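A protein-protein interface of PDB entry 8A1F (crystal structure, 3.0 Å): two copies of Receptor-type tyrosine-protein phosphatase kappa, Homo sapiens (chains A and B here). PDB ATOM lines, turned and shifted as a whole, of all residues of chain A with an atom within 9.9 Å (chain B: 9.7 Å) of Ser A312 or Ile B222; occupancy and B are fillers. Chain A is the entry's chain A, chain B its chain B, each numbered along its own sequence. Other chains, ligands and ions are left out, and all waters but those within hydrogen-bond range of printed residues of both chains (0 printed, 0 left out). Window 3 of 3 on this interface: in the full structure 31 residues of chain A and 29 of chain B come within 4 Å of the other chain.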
ATOM      1  N   TYR A 306      -0.974 -35.941  14.862  1.00  0.00           N
ATOM      2  CA  TYR A 306      -1.695 -34.691  14.665  1.00  0.00           C
ATOM      3  C   TYR A 306      -0.993 -33.831  13.619  1.00  0.00           C
ATOM      4  O   TYR A 306       0.236 -33.842  13.500  1.00  0.00           O
ATOM      5  CB  TYR A 306      -1.877 -33.917  15.995  1.00  0.00           C
ATOM      6  CG  TYR A 306      -0.644 -33.259  16.581  1.00  0.00           C
ATOM      7  CD1 TYR A 306       0.251 -33.975  17.365  1.00  0.00           C
ATOM      8  CD2 TYR A 306      -0.403 -31.904  16.383  1.00  0.00           C
ATOM      9  CE1 TYR A 306       1.364 -33.365  17.919  1.00  0.00           C
ATOM     10  CE2 TYR A 306       0.706 -31.286  16.933  1.00  0.00           C
ATOM     11  CZ  TYR A 306       1.586 -32.020  17.699  1.00  0.00           C
ATOM     12  OH  TYR A 306       2.693 -31.420  18.252  1.00  0.00           O
ATOM     13  N   ARG A 307      -1.789 -33.077  12.859  1.00  0.00           N
ATOM     14  CA  ARG A 307      -1.278 -32.281  11.753  1.00  0.00           C
ATOM     15  C   ARG A 307      -2.046 -30.970  11.648  1.00  0.00           C
ATOM     16  O   ARG A 307      -3.233 -30.910  11.950  1.00  0.00           O
ATOM     17  CB  ARG A 307      -1.392 -33.058  10.430  1.00  0.00           C
ATOM     18  CG  ARG A 307      -2.823 -33.459  10.067  1.00  0.00           C
ATOM     19  CD  ARG A 307      -2.888 -34.285   8.792  1.00  0.00           C
ATOM     20  NE  ARG A 307      -2.813 -35.717   9.059  1.00  0.00           N
ATOM     21  CZ  ARG A 307      -3.231 -36.655   8.220  1.00  0.00           C
ATOM     22  NH1 ARG A 307      -3.771 -36.347   7.052  1.00  0.00           N
ATOM     23  NH2 ARG A 307      -3.108 -37.934   8.565  1.00  0.00           N
ATOM     24  N   MET A 308      -1.368 -29.916  11.216  1.00  0.00           N
ATOM     25  CA  MET A 308      -2.086 -28.728  10.760  1.00  0.00           C
ATOM     26  C   MET A 308      -2.724 -29.034   9.398  1.00  0.00           C
ATOM     27  O   MET A 308      -2.171 -29.792   8.592  1.00  0.00           O
ATOM     28  CB  MET A 308      -1.130 -27.532  10.705  1.00  0.00           C
ATOM     29  CG  MET A 308      -0.650 -27.000  12.073  1.00  0.00           C
ATOM     30  SD  MET A 308       0.645 -25.728  11.925  1.00  0.00           S
ATOM     31  CE  MET A 308      -0.166 -24.423  10.992  1.00  0.00           C
ATOM     32  N   THR A 309      -3.926 -28.495   9.164  1.00  0.00           N
ATOM     33  CA  THR A 309      -4.636 -28.833   7.934  1.00  0.00           C
ATOM     34  C   THR A 309      -3.858 -28.350   6.717  1.00  0.00           C
ATOM     35  O   THR A 309      -3.862 -29.011   5.674  1.00  0.00           O
ATOM     36  CB  THR A 309      -6.044 -28.203   7.948  1.00  0.00           C
ATOM     37  OG1 THR A 309      -6.740 -28.588   9.132  1.00  0.00           O
ATOM     38  CG2 THR A 309      -6.859 -28.622   6.737  1.00  0.00           C
ATOM     39  N   SER A 310      -3.176 -27.205   6.836  1.00  0.00           N
ATOM     40  CA  SER A 310      -2.208 -26.737   5.848  1.00  0.00           C
ATOM     41  C   SER A 310      -0.857 -27.432   5.951  1.00  0.00           C
ATOM     42  O   SER A 310       0.001 -27.196   5.098  1.00  0.00           O
ATOM     43  CB  SER A 310      -2.017 -25.225   5.988  1.00  0.00           C
ATOM     44  OG  SER A 310      -1.744 -24.873   7.332  1.00  0.00           O
ATOM     45  N   GLY A 311      -0.646 -28.265   6.966  1.00  0.00           N
ATOM     46  CA  GLY A 311       0.686 -28.783   7.242  1.00  0.00           C
ATOM     47  C   GLY A 311       1.235 -29.715   6.172  1.00  0.00           C
ATOM     48  O   GLY A 311       0.513 -30.508   5.566  1.00  0.00           O
ATOM     49  N   SER A 312       2.550 -29.596   5.943  1.00  0.00           N
ATOM     50  CA  SER A 312       3.331 -30.517   5.125  1.00  0.00           C
ATOM     51  C   SER A 312       3.773 -31.757   5.894  1.00  0.00           C
ATOM     52  O   SER A 312       4.180 -32.747   5.274  1.00  0.00           O
ATOM     53  CB  SER A 312       4.562 -29.801   4.554  1.00  0.00           C
ATOM     54  OG  SER A 312       5.341 -29.217   5.582  1.00  0.00           O
ATOM     55  N   TRP A 313       3.700 -31.724   7.225  1.00  0.00           N
ATOM     56  CA  TRP A 313       4.240 -32.771   8.078  1.00  0.00           C
ATOM     57  C   TRP A 313       3.252 -33.115   9.185  1.00  0.00           C
ATOM     58  O   TRP A 313       2.349 -32.340   9.509  1.00  0.00           O
ATOM     59  CB  TRP A 313       5.573 -32.348   8.701  1.00  0.00           C
ATOM     60  CG  TRP A 313       5.504 -31.005   9.358  1.00  0.00           C
ATOM     61  CD1 TRP A 313       5.879 -29.815   8.813  1.00  0.00           C
ATOM     62  CD2 TRP A 313       4.986 -30.703  10.662  1.00  0.00           C
ATOM     63  NE1 TRP A 313       5.661 -28.795   9.705  1.00  0.00           N
ATOM     64  CE2 TRP A 313       5.108 -29.312  10.845  1.00  0.00           C
ATOM     65  CE3 TRP A 313       4.445 -31.473  11.696  1.00  0.00           C
ATOM     66  CZ2 TRP A 313       4.707 -28.675  12.016  1.00  0.00           C
ATOM     67  CZ3 TRP A 313       4.046 -30.839  12.856  1.00  0.00           C
ATOM     68  CH2 TRP A 313       4.179 -29.454  13.007  1.00  0.00           C
ATOM     69  N   THR A 314       3.431 -34.310   9.752  1.00  0.00           N
ATOM     70  CA  THR A 314       2.576 -34.840  10.806  1.00  0.00           C
ATOM     71  C   THR A 314       3.432 -35.350  11.961  1.00  0.00           C
ATOM     72  O   THR A 314       4.476 -35.970  11.745  1.00  0.00           O
ATOM     73  CB  THR A 314       1.675 -35.971  10.273  1.00  0.00           C
ATOM     74  OG1 THR A 314       0.835 -35.461   9.229  1.00  0.00           O
ATOM     75  CG2 THR A 314       0.802 -36.542  11.383  1.00  0.00           C
ATOM     76  N   GLU A 315       2.979 -35.085  13.186  1.00  0.00           N
ATOM     77  CA  GLU A 315       3.702 -35.413  14.410  1.00  0.00           C
ATOM     78  C   GLU A 315       3.014 -36.581  15.105  1.00  0.00           C
ATOM     79  O   GLU A 315       1.807 -36.527  15.359  1.00  0.00           O
ATOM     80  CB  GLU A 315       3.751 -34.198  15.343  1.00  0.00           C
ATOM     81  CG  GLU A 315       4.564 -34.369  16.624  1.00  0.00           C
ATOM     82  CD  GLU A 315       6.060 -34.234  16.420  1.00  0.00           C
ATOM     83  OE1 GLU A 315       6.519 -34.253  15.259  1.00  0.00           O
ATOM     84  OE2 GLU A 315       6.780 -34.096  17.433  1.00  0.00           O
ATOM     85  N   LEU B 175       7.642 -27.727  20.510  1.00  0.00           N
ATOM     86  CA  LEU B 175       6.412 -28.491  20.641  1.00  0.00           C
ATOM     87  C   LEU B 175       6.597 -29.599  21.679  1.00  0.00           C
ATOM     88  O   LEU B 175       7.699 -29.836  22.185  1.00  0.00           O
ATOM     89  CB  LEU B 175       5.994 -29.077  19.289  1.00  0.00           C
ATOM     90  CG  LEU B 175       5.836 -28.087  18.131  1.00  0.00           C
ATOM     91  CD1 LEU B 175       5.320 -28.791  16.888  1.00  0.00           C
ATOM     92  CD2 LEU B 175       4.888 -26.972  18.528  1.00  0.00           C
ATOM     93  N   GLN B 191      13.187 -36.800  19.460  1.00  0.00           N
ATOM     94  CA  GLN B 191      13.074 -35.826  18.375  1.00  0.00           C
ATOM     95  C   GLN B 191      12.319 -34.592  18.853  1.00  0.00           C
ATOM     96  O   GLN B 191      11.180 -34.699  19.323  1.00  0.00           O
ATOM     97  CB  GLN B 191      12.376 -36.418  17.149  1.00  0.00           C
ATOM     98  CG  GLN B 191      12.155 -35.384  16.058  1.00  0.00           C
ATOM     99  CD  GLN B 191      12.483 -35.894  14.672  1.00  0.00           C
ATOM    100  OE1 GLN B 191      13.646 -35.944  14.274  1.00  0.00           O
ATOM    101  NE2 GLN B 191      11.454 -36.274  13.924  1.00  0.00           N
ATOM    102  N   CYS B 192      12.940 -33.425  18.709  1.00  0.00           N
ATOM    103  CA  CYS B 192      12.361 -32.160  19.138  1.00  0.00           C
ATOM    104  C   CYS B 192      12.040 -31.272  17.942  1.00  0.00           C
ATOM    105  O   CYS B 192      12.824 -31.185  16.993  1.00  0.00           O
ATOM    106  CB  CYS B 192      13.309 -31.433  20.089  1.00  0.00           C
ATOM    107  SG  CYS B 192      13.343 -32.184  21.719  1.00  0.00           S
ATOM    108  N   ILE B 193      10.883 -30.612  17.994  1.00  0.00           N
ATOM    109  CA  ILE B 193      10.437 -29.684  16.959  1.00  0.00           C
ATOM    110  C   ILE B 193      10.375 -28.291  17.569  1.00  0.00           C
ATOM    111  O   ILE B 193       9.753 -28.097  18.619  1.00  0.00           O
ATOM    112  CB  ILE B 193       9.067 -30.093  16.386  1.00  0.00           C
ATOM    113  CG1 ILE B 193       9.052 -31.584  16.041  1.00  0.00           C
ATOM    114  CG2 ILE B 193       8.720 -29.250  15.172  1.00  0.00           C
ATOM    115  CD1 ILE B 193      10.033 -31.973  14.968  1.00  0.00           C
ATOM    116  N   ALA B 194      11.015 -27.323  16.910  1.00  0.00           N
ATOM    117  CA  ALA B 194      11.107 -25.961  17.422  1.00  0.00           C
ATOM    118  C   ALA B 194      10.789 -24.936  16.340  1.00  0.00           C
ATOM    119  O   ALA B 194      11.154 -25.109  15.174  1.00  0.00           O
ATOM    120  CB  ALA B 194      12.496 -25.666  17.993  1.00  0.00           C
ATOM    121  N   THR B 195      10.113 -23.865  16.741  1.00  0.00           N
ATOM    122  CA  THR B 195       9.909 -22.702  15.898  1.00  0.00           C
ATOM    123  C   THR B 195      11.077 -21.731  16.033  1.00  0.00           C
ATOM    124  O   THR B 195      11.685 -21.606  17.097  1.00  0.00           O
ATOM    125  CB  THR B 195       8.608 -21.983  16.258  1.00  0.00           C
ATOM    126  OG1 THR B 195       8.765 -21.305  17.510  1.00  0.00           O
ATOM    127  CG2 THR B 195       7.457 -22.968  16.362  1.00  0.00           C
ATOM    128  N   GLY B 196      11.389 -21.036  14.940  1.00  0.00           N
ATOM    129  CA  GLY B 196      12.422 -20.025  14.949  1.00  0.00           C
ATOM    130  C   GLY B 196      13.381 -20.189  13.792  1.00  0.00           C
ATOM    131  O   GLY B 196      13.146 -20.963  12.859  1.00  0.00           O
ATOM    132  N   ARG B 197      14.475 -19.434  13.851  1.00  0.00           N
ATOM    133  CA  ARG B 197      15.401 -19.282  12.724  1.00  0.00           C
ATOM    134  C   ARG B 197      15.938 -20.597  12.150  1.00  0.00           C
ATOM    135  O   ARG B 197      16.073 -21.601  12.847  1.00  0.00           O
ATOM    136  CB  ARG B 197      16.579 -18.396  13.140  1.00  0.00           C
ATOM    137  CG  ARG B 197      17.410 -18.935  14.295  1.00  0.00           C
ATOM    138  CD  ARG B 197      18.643 -18.073  14.528  1.00  0.00           C
ATOM    139  NE  ARG B 197      19.509 -18.031  13.355  1.00  0.00           N
ATOM    140  CZ  ARG B 197      20.513 -18.868  13.134  1.00  0.00           C
ATOM    141  NH1 ARG B 197      20.818 -19.826  13.995  1.00  0.00           N
ATOM    142  NH2 ARG B 197      21.231 -18.742  12.021  1.00  0.00           N
ATOM    143  N   THR B 219      20.261 -32.769  12.605  1.00  0.00           N
ATOM    144  CA  THR B 219      19.317 -31.657  12.518  1.00  0.00           C
ATOM    145  C   THR B 219      18.897 -31.450  11.064  1.00  0.00           C
ATOM    146  O   THR B 219      19.737 -31.490  10.161  1.00  0.00           O
ATOM    147  CB  THR B 219      19.943 -30.371  13.083  1.00  0.00           C
ATOM    148  OG1 THR B 219      20.392 -30.601  14.427  1.00  0.00           O
ATOM    149  CG2 THR B 219      18.947 -29.228  13.078  1.00  0.00           C
ATOM    150  N   LYS B 220      17.596 -31.221  10.845  1.00  0.00           N
ATOM    151  CA  LYS B 220      17.025 -31.032   9.514  1.00  0.00           C
ATOM    152  C   LYS B 220      15.924 -29.971   9.538  1.00  0.00           C
ATOM    153  O   LYS B 220      15.358 -29.657  10.587  1.00  0.00           O
ATOM    154  CB  LYS B 220      16.492 -32.354   8.944  1.00  0.00           C
ATOM    155  CG  LYS B 220      17.016 -32.679   7.550  1.00  0.00           C
ATOM    156  CD  LYS B 220      16.217 -31.958   6.470  1.00  0.00           C
ATOM    157  CE  LYS B 220      16.678 -32.341   5.071  1.00  0.00           C
ATOM    158  NZ  LYS B 220      15.784 -31.770   4.023  1.00  0.00           N
ATOM    159  N   ASN B 221      15.632 -29.416   8.355  1.00  0.00           N
ATOM    160  CA  ASN B 221      14.587 -28.408   8.147  1.00  0.00           C
ATOM    161  C   ASN B 221      13.281 -29.023   7.644  1.00  0.00           C
ATOM    162  O   ASN B 221      13.237 -29.575   6.536  1.00  0.00           O
ATOM    163  CB  ASN B 221      15.027 -27.347   7.139  1.00  0.00           C
ATOM    164  CG  ASN B 221      16.336 -26.695   7.502  1.00  0.00           C
ATOM    165  OD1 ASN B 221      16.559 -26.323   8.652  1.00  0.00           O
ATOM    166  ND2 ASN B 221      17.203 -26.520   6.508  1.00  0.00           N
ATOM    167  N   ILE B 222      12.238 -28.983   8.483  1.00  0.00           N
ATOM    168  CA  ILE B 222      10.927 -29.519   8.110  1.00  0.00           C
ATOM    169  C   ILE B 222       9.956 -28.449   7.604  1.00  0.00           C
ATOM    170  O   ILE B 222       8.930 -28.804   7.002  1.00  0.00           O
ATOM    171  CB  ILE B 222      10.264 -30.272   9.283  1.00  0.00           C
ATOM    172  CG1 ILE B 222       9.868 -29.291  10.389  1.00  0.00           C
ATOM    173  CG2 ILE B 222      11.189 -31.357   9.821  1.00  0.00           C
ATOM    174  CD1 ILE B 222       9.070 -29.907  11.508  1.00  0.00           C
ATOM    175  N   ASN B 223      10.248 -27.161   7.807  1.00  0.00           N
ATOM    176  CA  ASN B 223       9.293 -26.094   7.519  1.00  0.00           C
ATOM    177  C   ASN B 223      10.038 -24.768   7.435  1.00  0.00           C
ATOM    178  O   ASN B 223      11.197 -24.661   7.844  1.00  0.00           O
ATOM    179  CB  ASN B 223       8.206 -26.055   8.606  1.00  0.00           C
ATOM    180  CG  ASN B 223       7.160 -24.971   8.376  1.00  0.00           C
ATOM    181  OD1 ASN B 223       7.076 -24.003   9.137  1.00  0.00           O
ATOM    182  ND2 ASN B 223       6.360 -25.129   7.332  1.00  0.00           N
ATOM    183  N   HIS B 224       9.357 -23.751   6.890  1.00  0.00           N
ATOM    184  CA  HIS B 224       9.939 -22.410   6.846  1.00  0.00           C
ATOM    185  C   HIS B 224      10.065 -21.816   8.247  1.00  0.00           C
ATOM    186  O   HIS B 224      11.045 -21.124   8.548  1.00  0.00           O
ATOM    187  CB  HIS B 224       9.113 -21.493   5.934  1.00  0.00           C
ATOM    188  CG  HIS B 224       7.799 -21.070   6.515  1.00  0.00           C
ATOM    189  ND1 HIS B 224       6.692 -21.891   6.531  1.00  0.00           N
ATOM    190  CD2 HIS B 224       7.413 -19.906   7.091  1.00  0.00           C
ATOM    191  CE1 HIS B 224       5.682 -21.254   7.096  1.00  0.00           C
ATOM    192  NE2 HIS B 224       6.093 -20.048   7.446  1.00  0.00           N
ATOM    193  N   ARG B 225       9.090 -22.088   9.118  1.00  0.00           N
ATOM    194  CA  ARG B 225       9.079 -21.552  10.475  1.00  0.00           C
ATOM    195  C   ARG B 225       9.610 -22.518  11.527  1.00  0.00           C
ATOM    196  O   ARG B 225      10.000 -22.071  12.611  1.00  0.00           O
ATOM    197  CB  ARG B 225       7.659 -21.106  10.867  1.00  0.00           C
ATOM    198  CG  ARG B 225       7.596 -20.330  12.188  1.00  0.00           C
ATOM    199  CD  ARG B 225       6.225 -19.750  12.504  1.00  0.00           C
ATOM    200  NE  ARG B 225       5.927 -18.583  11.684  1.00  0.00           N
ATOM    201  CZ  ARG B 225       4.909 -17.760  11.899  1.00  0.00           C
ATOM    202  NH1 ARG B 225       4.051 -17.967  12.885  1.00  0.00           N
ATOM    203  NH2 ARG B 225       4.773 -16.682  11.131  1.00  0.00           N
ATOM    204  N   ARG B 226       9.674 -23.811  11.236  1.00  0.00           N
ATOM    205  CA  ARG B 226       9.985 -24.817  12.240  1.00  0.00           C
ATOM    206  C   ARG B 226      11.095 -25.729  11.744  1.00  0.00           C
ATOM    207  O   ARG B 226      11.161 -26.059  10.556  1.00  0.00           O
ATOM    208  CB  ARG B 226       8.759 -25.655  12.661  1.00  0.00           C
ATOM    209  CG  ARG B 226       7.668 -24.912  13.436  1.00  0.00           C
ATOM    210  CD  ARG B 226       6.349 -25.694  13.460  1.00  0.00           C
ATOM    211  NE  ARG B 226       5.399 -25.137  14.418  1.00  0.00           N
ATOM    212  CZ  ARG B 226       4.534 -24.158  14.178  1.00  0.00           C
ATOM    213  NH1 ARG B 226       4.549 -23.483  13.039  1.00  0.00           N
ATOM    214  NH2 ARG B 226       3.677 -23.804  15.132  1.00  0.00           N
ATOM    215  N   PHE B 227      11.963 -26.127  12.673  1.00  0.00           N
ATOM    216  CA  PHE B 227      13.071 -27.032  12.421  1.00  0.00           C
ATOM    217  C   PHE B 227      13.046 -28.169  13.435  1.00  0.00           C
ATOM    218  O   PHE B 227      12.377 -28.098  14.468  1.00  0.00           O
ATOM    219  CB  PHE B 227      14.410 -26.273  12.466  1.00  0.00           C
ATOM    220  CG  PHE B 227      14.867 -25.895  13.858  1.00  0.00           C
ATOM    221  CD1 PHE B 227      15.587 -26.781  14.646  1.00  0.00           C
ATOM    222  CD2 PHE B 227      14.594 -24.633  14.364  1.00  0.00           C
ATOM    223  CE1 PHE B 227      16.008 -26.418  15.919  1.00  0.00           C
ATOM    224  CE2 PHE B 227      15.015 -24.265  15.631  1.00  0.00           C
ATOM    225  CZ  PHE B 227      15.721 -25.158  16.409  1.00  0.00           C
ATOM    226  N   ALA B 228      13.795 -29.226  13.121  1.00  0.00           N
ATOM    227  CA  ALA B 228      13.764 -30.469  13.877  1.00  0.00           C
ATOM    228  C   ALA B 228      15.178 -30.908  14.231  1.00  0.00           C
ATOM    229  O   ALA B 228      16.126 -30.674  13.476  1.00  0.00           O
ATOM    230  CB  ALA B 228      13.061 -31.581  13.085  1.00  0.00           C
ATOM    231  N   ALA B 229      15.306 -31.565  15.385  1.00  0.00           N
ATOM    232  CA  ALA B 229      16.583 -32.099  15.842  1.00  0.00           C
ATOM    233  C   ALA B 229      16.380 -33.454  16.502  1.00  0.00           C
ATOM    234  O   ALA B 229      15.374 -33.677  17.180  1.00  0.00           O
ATOM    235  CB  ALA B 229      17.268 -31.149  16.826  1.00  0.00           C
ATOM    236  N   SER B 230      17.348 -34.353  16.308  1.00  0.00           N
ATOM    237  CA  SER B 230      17.249 -35.742  16.739  1.00  0.00           C
ATOM    238  C   SER B 230      18.438 -36.110  17.620  1.00  0.00           C
ATOM    239  O   SER B 230      19.568 -35.684  17.365  1.00  0.00           O
ATOM    240  CB  SER B 230      17.179 -36.691  15.535  1.00  0.00           C
ATOM    241  OG  SER B 230      16.361 -36.143  14.516  1.00  0.00           O
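Of the printed residues of chain B, Tyr A306 touches Leu B175 (3.96 Å). Of chain B, only Ile B222 (3.9 Å) comes within 4 Å of Ser A312. Trp A313 touches just these residues of chain B: Ile B222, Asn B223 and Arg B226. Of the printed residues of chain B, Glu A315 touches Ile B193. Printed residues of chain A within 4 Å of Leu B175: Tyr A306 (3.96 Å). Of the printed residues of chain A, Ile B193 touches Glu A315. Of chain A, only Ser A312 (3.9 Å) and Trp A313 (3.7 Å) come within 4 Å of Ile B222. Of chain A, only Trp A313 (3.9 Å) comes within 4 Å of Asn B223. Printed residues of chain A within 4 Å of Arg B226: Trp A313 (3.7 Å). The nearest residue of chain A that does not touch Ile B222 is Glu A315 (6.3 Å). The nearest printed residue of chain B that does not touch Glu A315 is Gln B191 (4.8 Å).
No position is printed for both chains.
Hydrophobic or aromatic side chains of chain A that line the printed part of chain B: Tyr A306 and Trp A313. Of the 20 printed residues of chain B, 5 touch a printed residue of chain A. Printed residues of chain B that touch a printed residue of chain A: Leu B175, Ile B193, Ile B222, Asn B223 and Arg B226. Hydrophobic or aromatic side chains of chain B within 4 Å of the printed part of chain A: Leu B175 and Ile B193. Among the printed residues, no Asp or Glu carboxylate lies within 4 Å of a Lys or Arg side-chain nitrogen of the other chain.
The backbone NH (N) of Tyr A306 lies within hydrogen-bond range of the backbone carbonyl oxygen (O) of Glu A315, 2.9 Å away. N of Leu B175 is in hydrogen-bond range of O of Ile B193 (2.9 Å). A ring nitrogen (ND1) of His B224 is in hydrogen-bond range of the side-chain amide nitrogen (ND2) of Asn B223, at 3.4 Å. OD1 of Asn B223 sits at hydrogen-bond distance from N of Arg B225. N of Arg B226 sits at hydrogen-bond distance from OD1 of Asn B223, at 3.3 Å.
Leu B175 touches Tyr A306. Ser A312 touches Ile B222. Trp A313 touches Ile B222. Trp A313 touches Asn B223 (NE1 to CB, 3.9 Å). CZ2 of Trp A313 touches CD of Arg B226, 3.7 Å away. OE2 of Glu A315 touches CG1 of Ile B193 (3.7 Å).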
